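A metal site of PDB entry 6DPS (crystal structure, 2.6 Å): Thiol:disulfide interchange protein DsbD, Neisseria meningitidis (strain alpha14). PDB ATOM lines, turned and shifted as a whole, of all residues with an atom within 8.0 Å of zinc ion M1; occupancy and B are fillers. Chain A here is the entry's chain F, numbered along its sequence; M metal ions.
Merely in contact with zinc ion M1: Tyr 35 (3.8 Å). Four residues have an atom within 4 Å of zinc ion M1: Tyr 35, Lys 62, His 74 and Glu 102. The nearest printed residue that does not touch zinc ion M1 is Val 72 (5.2 Å).
Zinc ion M1 is bound by OE2 of Glu 102, NZ of Lys 62 and NE2 of His 74. Zinc ion M1 has three donor atoms within binding distance.
O of Tyr 35 sits at hydrogen-bond distance from N of Cys 100 (2.9 Å). ND1 of His 74 sits at hydrogen-bond distance from OE2 of Glu 60, at 3.2 Å. The side-chain hydroxyl of Tyr 35 sits at hydrogen-bond distance from the side-chain carboxylate of Asp 64 (2.9 Å). The backbone NH of Glu 102 sits at hydrogen-bond distance from the backbone carbonyl oxygen of Gly 33, 2.8 Å away.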
ATOM      1  N   GLY A  33     -20.611  -4.853 -25.155  1.00  0.00           N
ATOM      2  CA  GLY A  33     -19.712  -3.732 -25.297  1.00  0.00           C
ATOM      3  C   GLY A  33     -18.240  -4.071 -25.171  1.00  0.00           C
ATOM      4  O   GLY A  33     -17.414  -3.157 -25.161  1.00  0.00           O
ATOM      5  N   TYR A  34     -17.904  -5.352 -25.103  1.00  0.00           N
ATOM      6  CA  TYR A  34     -16.548  -5.808 -24.864  1.00  0.00           C
ATOM      7  C   TYR A  34     -16.218  -6.865 -25.906  1.00  0.00           C
ATOM      8  O   TYR A  34     -17.105  -7.449 -26.520  1.00  0.00           O
ATOM      9  CB  TYR A  34     -16.394  -6.370 -23.421  1.00  0.00           C
ATOM     10  CG  TYR A  34     -16.584  -5.305 -22.369  1.00  0.00           C
ATOM     11  CD1 TYR A  34     -17.856  -4.917 -21.967  1.00  0.00           C
ATOM     12  CD2 TYR A  34     -15.484  -4.671 -21.788  1.00  0.00           C
ATOM     13  CE1 TYR A  34     -18.036  -3.921 -20.995  1.00  0.00           C
ATOM     14  CE2 TYR A  34     -15.652  -3.668 -20.814  1.00  0.00           C
ATOM     15  CZ  TYR A  34     -16.932  -3.307 -20.423  1.00  0.00           C
ATOM     16  OH  TYR A  34     -17.098  -2.315 -19.478  1.00  0.00           O
ATOM     17  N   TYR A  35     -14.924  -7.112 -26.107  1.00  0.00           N
ATOM     18  CA  TYR A  35     -14.529  -8.173 -27.034  1.00  0.00           C
ATOM     19  C   TYR A  35     -13.201  -8.770 -26.594  1.00  0.00           C
ATOM     20  O   TYR A  35     -12.394  -8.110 -25.944  1.00  0.00           O
ATOM     21  CB  TYR A  35     -14.462  -7.657 -28.480  1.00  0.00           C
ATOM     22  CG  TYR A  35     -13.457  -6.567 -28.728  1.00  0.00           C
ATOM     23  CD1 TYR A  35     -13.773  -5.217 -28.485  1.00  0.00           C
ATOM     24  CD2 TYR A  35     -12.183  -6.880 -29.194  1.00  0.00           C
ATOM     25  CE1 TYR A  35     -12.841  -4.207 -28.707  1.00  0.00           C
ATOM     26  CE2 TYR A  35     -11.230  -5.861 -29.426  1.00  0.00           C
ATOM     27  CZ  TYR A  35     -11.563  -4.540 -29.184  1.00  0.00           C
ATOM     28  OH  TYR A  35     -10.616  -3.584 -29.424  1.00  0.00           O
ATOM     29  N   MET A  36     -12.998 -10.042 -26.954  1.00  0.00           N
ATOM     30  CA  MET A  36     -11.798 -10.796 -26.609  1.00  0.00           C
ATOM     31  C   MET A  36     -10.953 -11.053 -27.852  1.00  0.00           C
ATOM     32  O   MET A  36     -11.494 -11.369 -28.911  1.00  0.00           O
ATOM     33  CB  MET A  36     -12.157 -12.140 -25.977  1.00  0.00           C
ATOM     34  CG  MET A  36     -12.652 -12.056 -24.546  1.00  0.00           C
ATOM     35  SD  MET A  36     -13.007 -13.676 -23.815  1.00  0.00           S
ATOM     36  CE  MET A  36     -11.342 -14.250 -23.581  1.00  0.00           C
ATOM     37  N   GLU A  60     -14.942 -13.678 -35.134  1.00  0.00           N
ATOM     38  CA  GLU A  60     -15.182 -12.556 -36.043  1.00  0.00           C
ATOM     39  C   GLU A  60     -13.904 -11.784 -36.310  1.00  0.00           C
ATOM     40  O   GLU A  60     -12.971 -11.773 -35.502  1.00  0.00           O
ATOM     41  CB  GLU A  60     -16.247 -11.588 -35.501  1.00  0.00           C
ATOM     42  CG  GLU A  60     -17.541 -12.285 -35.138  1.00  0.00           C
ATOM     43  CD  GLU A  60     -18.358 -11.518 -34.129  1.00  0.00           C
ATOM     44  OE1 GLU A  60     -18.634 -12.074 -33.027  1.00  0.00           O
ATOM     45  OE2 GLU A  60     -18.721 -10.360 -34.435  1.00  0.00           O
ATOM     46  N   GLU A  61     -13.874 -11.106 -37.459  1.00  0.00           N
ATOM     47  CA  GLU A  61     -12.688 -10.401 -37.940  1.00  0.00           C
ATOM     48  C   GLU A  61     -12.813  -8.916 -37.674  1.00  0.00           C
ATOM     49  O   GLU A  61     -13.841  -8.305 -37.951  1.00  0.00           O
ATOM     50  CB  GLU A  61     -12.484 -10.664 -39.427  1.00  0.00           C
ATOM     51  CG  GLU A  61     -12.071 -12.085 -39.682  1.00  0.00           C
ATOM     52  CD  GLU A  61     -10.883 -12.481 -38.835  1.00  0.00           C
ATOM     53  OE1 GLU A  61      -9.923 -11.702 -38.749  1.00  0.00           O
ATOM     54  OE2 GLU A  61     -10.924 -13.581 -38.230  1.00  0.00           O
ATOM     55  N   LYS A  62     -11.745  -8.328 -37.145  1.00  0.00           N
ATOM     56  CA  LYS A  62     -11.795  -6.914 -36.800  1.00  0.00           C
ATOM     57  C   LYS A  62     -10.408  -6.300 -36.945  1.00  0.00           C
ATOM     58  O   LYS A  62      -9.408  -6.929 -36.584  1.00  0.00           O
ATOM     59  CB  LYS A  62     -12.302  -6.687 -35.375  1.00  0.00           C
ATOM     60  CG  LYS A  62     -11.865  -5.362 -34.770  1.00  0.00           C
ATOM     61  CD  LYS A  62     -12.249  -5.236 -33.307  1.00  0.00           C
ATOM     62  CE  LYS A  62     -13.760  -5.285 -33.138  1.00  0.00           C
ATOM     63  NZ  LYS A  62     -14.181  -4.949 -31.759  1.00  0.00           N
ATOM     64  N   ASP A  64      -8.621  -3.027 -35.428  1.00  0.00           N
ATOM     65  CA  ASP A  64      -8.720  -1.960 -34.442  1.00  0.00           C
ATOM     66  C   ASP A  64      -7.393  -1.227 -34.308  1.00  0.00           C
ATOM     67  O   ASP A  64      -6.365  -1.634 -34.849  1.00  0.00           O
ATOM     68  CB  ASP A  64      -9.211  -2.479 -33.073  1.00  0.00           C
ATOM     69  CG  ASP A  64      -8.236  -3.451 -32.397  1.00  0.00           C
ATOM     70  OD1 ASP A  64      -7.045  -3.500 -32.735  1.00  0.00           O
ATOM     71  OD2 ASP A  64      -8.686  -4.184 -31.486  1.00  0.00           O
ATOM     72  N   VAL A  72     -11.598 -11.864 -33.202  1.00  0.00           N
ATOM     73  CA  VAL A  72     -12.078 -11.491 -31.888  1.00  0.00           C
ATOM     74  C   VAL A  72     -13.417 -12.175 -31.648  1.00  0.00           C
ATOM     75  O   VAL A  72     -14.020 -12.751 -32.549  1.00  0.00           O
ATOM     76  CB  VAL A  72     -12.200  -9.960 -31.700  1.00  0.00           C
ATOM     77  CG1 VAL A  72     -10.883  -9.300 -31.972  1.00  0.00           C
ATOM     78  CG2 VAL A  72     -13.289  -9.385 -32.605  1.00  0.00           C
ATOM     79  N   TYR A  73     -13.872 -12.112 -30.400  1.00  0.00           N
ATOM     80  CA  TYR A  73     -15.135 -12.695 -30.007  1.00  0.00           C
ATOM     81  C   TYR A  73     -16.017 -11.616 -29.408  1.00  0.00           C
ATOM     82  O   TYR A  73     -15.540 -10.652 -28.795  1.00  0.00           O
ATOM     83  CB  TYR A  73     -14.947 -13.825 -28.995  1.00  0.00           C
ATOM     84  CG  TYR A  73     -14.324 -15.060 -29.574  1.00  0.00           C
ATOM     85  CD1 TYR A  73     -15.070 -15.909 -30.380  1.00  0.00           C
ATOM     86  CD2 TYR A  73     -12.997 -15.381 -29.311  1.00  0.00           C
ATOM     87  CE1 TYR A  73     -14.515 -17.060 -30.922  1.00  0.00           C
ATOM     88  CE2 TYR A  73     -12.431 -16.539 -29.846  1.00  0.00           C
ATOM     89  CZ  TYR A  73     -13.197 -17.379 -30.657  1.00  0.00           C
ATOM     90  OH  TYR A  73     -12.688 -18.530 -31.216  1.00  0.00           O
ATOM     91  N   HIS A  74     -17.319 -11.782 -29.601  1.00  0.00           N
ATOM     92  CA  HIS A  74     -18.329 -10.958 -28.956  1.00  0.00           C
ATOM     93  C   HIS A  74     -19.327 -11.895 -28.298  1.00  0.00           C
ATOM     94  O   HIS A  74     -19.701 -12.918 -28.906  1.00  0.00           O
ATOM     95  CB  HIS A  74     -19.016 -10.022 -29.952  1.00  0.00           C
ATOM     96  CG  HIS A  74     -18.131  -8.977 -30.567  1.00  0.00           C
ATOM     97  ND1 HIS A  74     -17.439  -9.182 -31.744  1.00  0.00           N
ATOM     98  CD2 HIS A  74     -17.869  -7.700 -30.190  1.00  0.00           C
ATOM     99  CE1 HIS A  74     -16.769  -8.085 -32.052  1.00  0.00           C
ATOM    100  NE2 HIS A  74     -17.019  -7.173 -31.124  1.00  0.00           N
ATOM    101  N   CYS A 100     -10.881  -6.072 -24.614  1.00  0.00           N
ATOM    102  CA  CYS A 100     -10.978  -4.625 -24.707  1.00  0.00           C
ATOM    103  C   CYS A 100     -12.441  -4.234 -24.606  1.00  0.00           C
ATOM    104  O   CYS A 100     -13.349  -5.065 -24.690  1.00  0.00           O
ATOM    105  CB  CYS A 100     -10.382  -4.121 -26.016  1.00  0.00           C
ATOM    106  SG  CYS A 100      -8.671  -4.611 -26.273  1.00  0.00           S
ATOM    107  N   ALA A 101     -12.676  -2.944 -24.413  1.00  0.00           N
ATOM    108  CA  ALA A 101     -14.011  -2.382 -24.422  1.00  0.00           C
ATOM    109  C   ALA A 101     -14.204  -1.586 -25.700  1.00  0.00           C
ATOM    110  O   ALA A 101     -13.302  -0.833 -26.091  1.00  0.00           O
ATOM    111  CB  ALA A 101     -14.229  -1.478 -23.200  1.00  0.00           C
ATOM    112  N   GLU A 102     -15.358  -1.756 -26.360  1.00  0.00           N
ATOM    113  CA  GLU A 102     -15.640  -1.055 -27.619  1.00  0.00           C
ATOM    114  C   GLU A 102     -15.385   0.440 -27.537  1.00  0.00           C
ATOM    115  O   GLU A 102     -14.965   1.053 -28.514  1.00  0.00           O
ATOM    116  CB  GLU A 102     -17.084  -1.289 -28.064  1.00  0.00           C
ATOM    117  CG  GLU A 102     -17.438  -2.719 -28.372  1.00  0.00           C
ATOM    118  CD  GLU A 102     -16.707  -3.280 -29.595  1.00  0.00           C
ATOM    119  OE1 GLU A 102     -15.985  -2.530 -30.281  1.00  0.00           O
ATOM    120  OE2 GLU A 102     -16.891  -4.492 -29.871  1.00  0.00           O
HETATM  121 ZN    ZN M   1     -16.198  -5.281 -31.471  1.00  0.00          ZN
HETATM  122 ZN    ZN M   2     -22.331  -9.804 -31.645  1.00  0.00          ZN
